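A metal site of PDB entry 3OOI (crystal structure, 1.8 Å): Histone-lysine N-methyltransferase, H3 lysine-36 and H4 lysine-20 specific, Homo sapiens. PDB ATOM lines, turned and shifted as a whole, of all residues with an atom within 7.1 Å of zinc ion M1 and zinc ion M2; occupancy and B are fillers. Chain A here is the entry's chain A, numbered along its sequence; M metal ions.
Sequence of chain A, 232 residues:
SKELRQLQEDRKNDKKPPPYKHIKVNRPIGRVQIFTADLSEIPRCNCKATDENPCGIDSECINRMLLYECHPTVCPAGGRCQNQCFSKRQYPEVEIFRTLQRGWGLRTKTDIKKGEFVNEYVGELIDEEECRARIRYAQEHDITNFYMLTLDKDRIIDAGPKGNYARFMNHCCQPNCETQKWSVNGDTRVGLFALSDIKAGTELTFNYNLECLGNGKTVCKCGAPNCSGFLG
SG of Cys 75 lies close to N of Ala 77, at 3.3 Å. N of Asn 63 sits close to SG of Cys 61, 3.6 Å away. The backbone NH (N) of Cys 61 lies close to the side-chain hydroxyl (OG) of Ser 59, at 3.3 Å. The backbone carbonyl oxygen of Asn 83 lies within hydrogen-bond range of the backbone NH of Cys 70 (3.1 Å). The side-chain sulfur (SG) of Cys 70 sits close to the side-chain amide oxygen (OD1) of Asn 63, at 3.6 Å. O of Cys 55 is in hydrogen-bond range of NE of Arg 64 (2.9 Å). The side-chain sulfur (SG) of Cys 81 sits close to the backbone NH (N) of Asn 83, at 3.4 Å. The side-chain sulfur of Cys 81 lies close to the side-chain amide nitrogen of Gln 84.
Zinc ion M1 is bound by the side-chain sulfur (SG) of Cys 45 (2.3 Å), the side-chain sulfur (SG) of Cys 61 (2.3 Å), the side-chain sulfur (SG) of Cys 55 (2.4 Å) and the side-chain sulfur (SG) of Cys 47 (2.4 Å). Zinc ion M1 has four donor atoms within binding distance.
Zinc ion M2 is bound by the side-chain sulfur of Cys 75 (2.3 Å), the side-chain sulfur of Cys 70 (2.3 Å), the side-chain sulfur of Cys 81 (2.4 Å) and the side-chain sulfur of Cys 55 (2.4 Å). Zinc ion M2 has four donor atoms within binding distance.
Of the 29 residues printed, 4 come within 4 Å of zinc ion M2. The nearest printed residue that does not touch zinc ion M2 is Cys 45 (4.1 Å).
Four residues have an atom within 4 Å of zinc ion M1: Cys 45, Cys 47, Cys 55 and Cys 61.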
ATOM      1  N   ARG A  44      23.251  12.828  -8.921  1.00  0.00           N
ATOM      2  CA  ARG A  44      22.544  11.721  -8.286  1.00  0.00           C
ATOM      3  C   ARG A  44      23.619  10.745  -7.839  1.00  0.00           C
ATOM      4  O   ARG A  44      24.459  10.345  -8.649  1.00  0.00           O
ATOM      5  CB  ARG A  44      21.621  11.017  -9.277  1.00  0.00           C
ATOM      6  CG  ARG A  44      20.355  11.792  -9.673  1.00  0.00           C
ATOM      7  CD  ARG A  44      19.588  10.991 -10.731  1.00  0.00           C
ATOM      8  NE  ARG A  44      18.245  11.515 -11.011  1.00  0.00           N
ATOM      9  CZ  ARG A  44      17.986  12.441 -11.927  1.00  0.00           C
ATOM     10  NH1 ARG A  44      18.977  12.974 -12.639  1.00  0.00           N
ATOM     11  NH2 ARG A  44      16.734  12.848 -12.135  1.00  0.00           N
ATOM     12  N   CYS A  45      23.600  10.372  -6.566  1.00  0.00           N
ATOM     13  CA  CYS A  45      24.582   9.432  -6.016  1.00  0.00           C
ATOM     14  C   CYS A  45      24.236   7.968  -6.294  1.00  0.00           C
ATOM     15  O   CYS A  45      23.235   7.635  -6.945  1.00  0.00           O
ATOM     16  CB  CYS A  45      24.721   9.642  -4.511  1.00  0.00           C
ATOM     17  SG  CYS A  45      23.251   9.036  -3.601  1.00  0.00           S
ATOM     18  N   ASN A  46      25.114   7.095  -5.794  1.00  0.00           N
ATOM     19  CA  ASN A  46      25.045   5.642  -5.960  1.00  0.00           C
ATOM     20  C   ASN A  46      24.245   4.932  -4.868  1.00  0.00           C
ATOM     21  O   ASN A  46      24.115   3.715  -4.902  1.00  0.00           O
ATOM     22  CB  ASN A  46      26.477   5.067  -6.032  1.00  0.00           C
ATOM     23  CG  ASN A  46      27.363   5.532  -4.879  1.00  0.00           C
ATOM     24  OD1 ASN A  46      27.372   6.729  -4.514  1.00  0.00           O
ATOM     25  ND2 ASN A  46      28.119   4.598  -4.280  1.00  0.00           N
ATOM     26  N   CYS A  47      23.696   5.679  -3.912  1.00  0.00           N
ATOM     27  CA  CYS A  47      22.952   5.053  -2.808  1.00  0.00           C
ATOM     28  C   CYS A  47      21.559   4.609  -3.225  1.00  0.00           C
ATOM     29  O   CYS A  47      20.964   5.182  -4.149  1.00  0.00           O
ATOM     30  CB  CYS A  47      22.851   5.966  -1.583  1.00  0.00           C
ATOM     31  SG  CYS A  47      24.465   6.497  -0.957  1.00  0.00           S
ATOM     32  N   LYS A  48      21.050   3.602  -2.528  1.00  0.00           N
ATOM     33  CA  LYS A  48      19.720   3.087  -2.801  1.00  0.00           C
ATOM     34  C   LYS A  48      18.888   3.222  -1.535  1.00  0.00           C
ATOM     35  O   LYS A  48      19.433   3.197  -0.420  1.00  0.00           O
ATOM     36  CB  LYS A  48      19.785   1.625  -3.262  1.00  0.00           C
ATOM     37  CG  LYS A  48      20.613   1.365  -4.549  1.00  0.00           C
ATOM     38  CD  LYS A  48      20.181   2.246  -5.733  1.00  0.00           C
ATOM     39  CE  LYS A  48      21.000   1.966  -6.999  1.00  0.00           C
ATOM     40  NZ  LYS A  48      22.394   2.482  -6.971  1.00  0.00           N
ATOM     41  N   ASP A  51      19.444   0.710   1.312  1.00  0.00           N
ATOM     42  CA  ASP A  51      20.710   0.644   2.028  1.00  0.00           C
ATOM     43  C   ASP A  51      20.474   0.926   3.504  1.00  0.00           C
ATOM     44  O   ASP A  51      19.477   1.563   3.851  1.00  0.00           O
ATOM     45  CB  ASP A  51      21.738   1.631   1.468  1.00  0.00           C
ATOM     46  CG  ASP A  51      22.178   1.288   0.032  1.00  0.00           C
ATOM     47  OD1 ASP A  51      21.945   0.146  -0.444  1.00  0.00           O
ATOM     48  OD2 ASP A  51      22.777   2.169  -0.615  1.00  0.00           O
ATOM     49  N   ASN A  53      21.963   2.958   5.781  1.00  0.00           N
ATOM     50  CA  ASN A  53      21.980   4.379   6.133  1.00  0.00           C
ATOM     51  C   ASN A  53      22.346   5.174   4.901  1.00  0.00           C
ATOM     52  O   ASN A  53      23.497   5.617   4.764  1.00  0.00           O
ATOM     53  CB  ASN A  53      22.993   4.658   7.261  1.00  0.00           C
ATOM     54  CG  ASN A  53      22.499   4.211   8.627  1.00  0.00           C
ATOM     55  OD1 ASN A  53      21.600   4.829   9.216  1.00  0.00           O
ATOM     56  ND2 ASN A  53      23.087   3.134   9.152  1.00  0.00           N
ATOM     57  N   PRO A  54      21.386   5.338   3.972  1.00  0.00           N
ATOM     58  CA  PRO A  54      21.660   5.928   2.662  1.00  0.00           C
ATOM     59  C   PRO A  54      22.276   7.325   2.786  1.00  0.00           C
ATOM     60  O   PRO A  54      21.750   8.171   3.529  1.00  0.00           O
ATOM     61  CB  PRO A  54      20.269   6.014   2.008  1.00  0.00           C
ATOM     62  CG  PRO A  54      19.392   5.087   2.785  1.00  0.00           C
ATOM     63  CD  PRO A  54      19.939   5.077   4.172  1.00  0.00           C
ATOM     64  N   CYS A  55      23.387   7.520   2.088  1.00  0.00           N
ATOM     65  CA  CYS A  55      24.126   8.791   2.044  1.00  0.00           C
ATOM     66  C   CYS A  55      24.651   9.199   3.420  1.00  0.00           C
ATOM     67  O   CYS A  55      25.014  10.352   3.620  1.00  0.00           O
ATOM     68  CB  CYS A  55      23.271   9.907   1.407  1.00  0.00           C
ATOM     69  SG  CYS A  55      22.330   9.365  -0.056  1.00  0.00           S
ATOM     70  N   GLY A  56      24.726   8.236   4.333  1.00  0.00           N
ATOM     71  CA  GLY A  56      25.216   8.499   5.682  1.00  0.00           C
ATOM     72  C   GLY A  56      26.725   8.558   5.749  1.00  0.00           C
ATOM     73  O   GLY A  56      27.419   8.232   4.767  1.00  0.00           O
ATOM     74  N   SER A  59      28.507   5.453   4.696  1.00  0.00           N
ATOM     75  CA  SER A  59      28.012   4.826   3.452  1.00  0.00           C
ATOM     76  C   SER A  59      28.986   4.992   2.293  1.00  0.00           C
ATOM     77  O   SER A  59      29.976   5.696   2.412  1.00  0.00           O
ATOM     78  CB  SER A  59      26.676   5.457   3.043  1.00  0.00           C
ATOM     79  OG  SER A  59      26.904   6.757   2.535  1.00  0.00           O
ATOM     80  N   GLU A  60      28.661   4.373   1.166  1.00  0.00           N
ATOM     81  CA  GLU A  60      29.509   4.430  -0.033  1.00  0.00           C
ATOM     82  C   GLU A  60      29.219   5.673  -0.881  1.00  0.00           C
ATOM     83  O   GLU A  60      29.685   5.784  -2.017  1.00  0.00           O
ATOM     84  CB  GLU A  60      29.302   3.167  -0.892  1.00  0.00           C
ATOM     85  CG  GLU A  60      29.601   1.826  -0.179  1.00  0.00           C
ATOM     86  CD  GLU A  60      29.115   0.587  -0.955  1.00  0.00           C
ATOM     87  OE1 GLU A  60      29.285  -0.533  -0.436  1.00  0.00           O
ATOM     88  OE2 GLU A  60      28.561   0.723  -2.078  1.00  0.00           O
ATOM     89  N   CYS A  61      28.427   6.600  -0.338  1.00  0.00           N
ATOM     90  CA  CYS A  61      27.869   7.712  -1.110  1.00  0.00           C
ATOM     91  C   CYS A  61      28.924   8.584  -1.804  1.00  0.00           C
ATOM     92  O   CYS A  61      29.757   9.184  -1.128  1.00  0.00           O
ATOM     93  CB  CYS A  61      27.031   8.607  -0.200  1.00  0.00           C
ATOM     94  SG  CYS A  61      26.119   9.939  -1.045  1.00  0.00           S
ATOM     95  N   ILE A  62      28.843   8.666  -3.123  1.00  0.00           N
ATOM     96  CA  ILE A  62      29.765   9.493  -3.918  1.00  0.00           C
ATOM     97  C   ILE A  62      29.536  10.982  -3.729  1.00  0.00           C
ATOM     98  O   ILE A  62      30.484  11.771  -3.850  1.00  0.00           O
ATOM     99  CB  ILE A  62      29.713   9.099  -5.427  1.00  0.00           C
ATOM    100  CG1 ILE A  62      30.898   9.704  -6.206  1.00  0.00           C
ATOM    101  CG2 ILE A  62      28.375   9.485  -6.053  1.00  0.00           C
ATOM    102  CD1 ILE A  62      32.288   9.359  -5.648  1.00  0.00           C
ATOM    103  N   ASN A  63      28.290  11.403  -3.484  1.00  0.00           N
ATOM    104  CA  ASN A  63      28.041  12.844  -3.277  1.00  0.00           C
ATOM    105  C   ASN A  63      28.756  13.265  -1.999  1.00  0.00           C
ATOM    106  O   ASN A  63      29.530  14.237  -1.992  1.00  0.00           O
ATOM    107  CB  ASN A  63      26.524  13.149  -3.186  1.00  0.00           C
ATOM    108  CG  ASN A  63      25.852  13.260  -4.569  1.00  0.00           C
ATOM    109  OD1 ASN A  63      24.642  13.551  -4.651  1.00  0.00           O
ATOM    110  ND2 ASN A  63      26.601  13.040  -5.638  1.00  0.00           N
ATOM    111  N   ARG A  64      28.524  12.522  -0.927  1.00  0.00           N
ATOM    112  CA  ARG A  64      29.212  12.784   0.321  1.00  0.00           C
ATOM    113  C   ARG A  64      30.744  12.740   0.155  1.00  0.00           C
ATOM    114  O   ARG A  64      31.447  13.613   0.653  1.00  0.00           O
ATOM    115  CB  ARG A  64      28.748  11.796   1.399  1.00  0.00           C
ATOM    116  CG  ARG A  64      29.538  11.885   2.687  1.00  0.00           C
ATOM    117  CD  ARG A  64      28.953  10.955   3.753  1.00  0.00           C
ATOM    118  NE  ARG A  64      27.634  11.390   4.247  1.00  0.00           N
ATOM    119  CZ  ARG A  64      27.442  12.361   5.134  1.00  0.00           C
ATOM    120  NH1 ARG A  64      28.468  13.068   5.619  1.00  0.00           N
ATOM    121  NH2 ARG A  64      26.205  12.646   5.522  1.00  0.00           N
ATOM    122  N   GLU A  69      26.233  18.117  -1.349  1.00  0.00           N
ATOM    123  CA  GLU A  69      25.025  17.807  -0.624  1.00  0.00           C
ATOM    124  C   GLU A  69      23.968  17.282  -1.604  1.00  0.00           C
ATOM    125  O   GLU A  69      23.869  17.771  -2.740  1.00  0.00           O
ATOM    126  CB  GLU A  69      24.534  19.048   0.123  1.00  0.00           C
ATOM    127  CG  GLU A  69      23.276  18.806   0.890  1.00  0.00           C
ATOM    128  CD  GLU A  69      23.163  19.693   2.098  1.00  0.00           C
ATOM    129  OE1 GLU A  69      22.146  20.374   2.202  1.00  0.00           O
ATOM    130  OE2 GLU A  69      24.076  19.673   2.944  1.00  0.00           O
ATOM    131  N   CYS A  70      23.224  16.235  -1.214  1.00  0.00           N
ATOM    132  CA  CYS A  70      22.122  15.745  -2.049  1.00  0.00           C
ATOM    133  C   CYS A  70      20.955  16.738  -2.010  1.00  0.00           C
ATOM    134  O   CYS A  70      20.808  17.479  -1.039  1.00  0.00           O
ATOM    135  CB  CYS A  70      21.600  14.386  -1.549  1.00  0.00           C
ATOM    136  SG  CYS A  70      22.808  13.006  -1.640  1.00  0.00           S
ATOM    137  N   HIS A  71      20.159  16.756  -3.066  1.00  0.00           N
ATOM    138  CA  HIS A  71      18.879  17.494  -3.052  1.00  0.00           C
ATOM    139  C   HIS A  71      17.718  16.523  -2.778  1.00  0.00           C
ATOM    140  O   HIS A  71      17.651  15.460  -3.387  1.00  0.00           O
ATOM    141  CB  HIS A  71      18.684  18.221  -4.363  1.00  0.00           C
ATOM    142  CG  HIS A  71      17.521  19.172  -4.340  1.00  0.00           C
ATOM    143  ND1 HIS A  71      17.677  20.523  -4.141  1.00  0.00           N
ATOM    144  CD2 HIS A  71      16.198  18.945  -4.411  1.00  0.00           C
ATOM    145  CE1 HIS A  71      16.486  21.097  -4.120  1.00  0.00           C
ATOM    146  NE2 HIS A  71      15.573  20.162  -4.278  1.00  0.00           N
ATOM    147  N   VAL A  74      15.774  14.957  -5.688  1.00  0.00           N
ATOM    148  CA  VAL A  74      16.630  14.280  -6.687  1.00  0.00           C
ATOM    149  C   VAL A  74      17.269  12.979  -6.160  1.00  0.00           C
ATOM    150  O   VAL A  74      17.414  12.000  -6.909  1.00  0.00           O
ATOM    151  CB  VAL A  74      17.723  15.266  -7.172  1.00  0.00           C
ATOM    152  CG1 VAL A  74      18.733  14.601  -8.124  1.00  0.00           C
ATOM    153  CG2 VAL A  74      17.066  16.464  -7.874  1.00  0.00           C
ATOM    154  N   CYS A  75      17.635  12.962  -4.873  1.00  0.00           N
ATOM    155  CA  CYS A  75      18.396  11.820  -4.362  1.00  0.00           C
ATOM    156  C   CYS A  75      17.665  10.487  -4.577  1.00  0.00           C
ATOM    157  O   CYS A  75      16.478  10.363  -4.269  1.00  0.00           O
ATOM    158  CB  CYS A  75      18.717  11.973  -2.877  1.00  0.00           C
ATOM    159  SG  CYS A  75      19.746  10.593  -2.309  1.00  0.00           S
ATOM    160  N   PRO A  76      18.371   9.477  -5.127  1.00  0.00           N
ATOM    161  CA  PRO A  76      17.738   8.153  -5.271  1.00  0.00           C
ATOM    162  C   PRO A  76      17.258   7.514  -3.977  1.00  0.00           C
ATOM    163  O   PRO A  76      16.384   6.648  -4.013  1.00  0.00           O
ATOM    164  CB  PRO A  76      18.852   7.307  -5.909  1.00  0.00           C
ATOM    165  CG  PRO A  76      19.620   8.302  -6.727  1.00  0.00           C
ATOM    166  CD  PRO A  76      19.679   9.531  -5.826  1.00  0.00           C
ATOM    167  N   ALA A  77      17.819   7.923  -2.840  1.00  0.00           N
ATOM    168  CA  ALA A  77      17.421   7.381  -1.544  1.00  0.00           C
ATOM    169  C   ALA A  77      16.157   8.065  -0.966  1.00  0.00           C
ATOM    170  O   ALA A  77      15.658   7.672   0.105  1.00  0.00           O
ATOM    171  CB  ALA A  77      18.575   7.459  -0.550  1.00  0.00           C
ATOM    172  N   GLY A  78      15.663   9.071  -1.672  1.00  0.00           N
ATOM    173  CA  GLY A  78      14.479   9.836  -1.233  1.00  0.00           C
ATOM    174  C   GLY A  78      14.624  10.366   0.174  1.00  0.00           C
ATOM    175  O   GLY A  78      15.701  10.847   0.567  1.00  0.00           O
ATOM    176  N   ARG A  80      15.040   8.917   2.837  1.00  0.00           N
ATOM    177  CA  ARG A  80      16.026   8.217   3.654  1.00  0.00           C
ATOM    178  C   ARG A  80      17.434   8.795   3.552  1.00  0.00           C
ATOM    179  O   ARG A  80      18.322   8.418   4.311  1.00  0.00           O
ATOM    180  CB  ARG A  80      15.998   6.721   3.341  1.00  0.00           C
ATOM    181  CG  ARG A  80      14.561   6.146   3.413  1.00  0.00           C
ATOM    182  CD  ARG A  80      14.448   4.851   4.171  1.00  0.00           C
ATOM    183  NE  ARG A  80      15.475   3.878   3.840  1.00  0.00           N
ATOM    184  CZ  ARG A  80      16.385   3.427   4.706  1.00  0.00           C
ATOM    185  NH1 ARG A  80      16.391   3.844   5.958  1.00  0.00           N
ATOM    186  NH2 ARG A  80      17.289   2.540   4.311  1.00  0.00           N
ATOM    187  N   CYS A  81      17.622   9.734   2.616  1.00  0.00           N
ATOM    188  CA  CYS A  81      18.918  10.400   2.397  1.00  0.00           C
ATOM    189  C   CYS A  81      19.428  11.073   3.668  1.00  0.00           C
ATOM    190  O   CYS A  81      18.708  11.879   4.272  1.00  0.00           O
ATOM    191  CB  CYS A  81      18.802  11.434   1.270  1.00  0.00           C
ATOM    192  SG  CYS A  81      20.272  12.464   1.039  1.00  0.00           S
ATOM    193  N   GLN A  82      20.666  10.762   4.055  1.00  0.00           N
ATOM    194  CA  GLN A  82      21.289  11.323   5.257  1.00  0.00           C
ATOM    195  C   GLN A  82      22.379  12.339   4.910  1.00  0.00           C
ATOM    196  O   GLN A  82      23.258  12.627   5.727  1.00  0.00           O
ATOM    197  CB  GLN A  82      21.844  10.210   6.146  1.00  0.00           C
ATOM    198  CG  GLN A  82      20.770   9.256   6.662  1.00  0.00           C
ATOM    199  CD  GLN A  82      21.341   8.178   7.568  1.00  0.00           C
ATOM    200  OE1 GLN A  82      22.486   8.272   8.020  1.00  0.00           O
ATOM    201  NE2 GLN A  82      20.535   7.147   7.833  1.00  0.00           N
ATOM    202  N   ASN A  83      22.306  12.901   3.708  1.00  0.00           N
ATOM    203  CA  ASN A  83      23.333  13.847   3.236  1.00  0.00           C
ATOM    204  C   ASN A  83      22.753  15.224   2.900  1.00  0.00           C
ATOM    205  O   ASN A  83      22.925  15.736   1.799  1.00  0.00           O
ATOM    206  CB  ASN A  83      24.056  13.243   2.025  1.00  0.00           C
ATOM    207  CG  ASN A  83      25.235  14.090   1.530  1.00  0.00           C
ATOM    208  OD1 ASN A  83      25.927  14.731   2.326  1.00  0.00           O
ATOM    209  ND2 ASN A  83      25.464  14.105   0.223  1.00  0.00           N
ATOM    210  N   GLN A  84      22.050  15.814   3.865  1.00  0.00           N
ATOM    211  CA  GLN A  84      21.467  17.165   3.685  1.00  0.00           C
ATOM    212  C   GLN A  84      21.784  18.013   4.919  1.00  0.00           C
ATOM    213  O   GLN A  84      20.948  18.781   5.384  1.00  0.00           O
ATOM    214  CB  GLN A  84      19.960  17.072   3.422  1.00  0.00           C
ATOM    215  CG  GLN A  84      19.637  16.389   2.080  1.00  0.00           C
ATOM    216  CD  GLN A  84      18.178  15.985   1.936  1.00  0.00           C
ATOM    217  OE1 GLN A  84      17.269  16.698   2.376  1.00  0.00           O
ATOM    218  NE2 GLN A  84      17.942  14.840   1.292  1.00  0.00           N
HETATM  219 ZN    ZN M   1      24.110   8.831  -1.495  1.00  0.00          ZN
HETATM  220 ZN    ZN M   2      21.327  11.399  -0.792  1.00  0.00          ZN
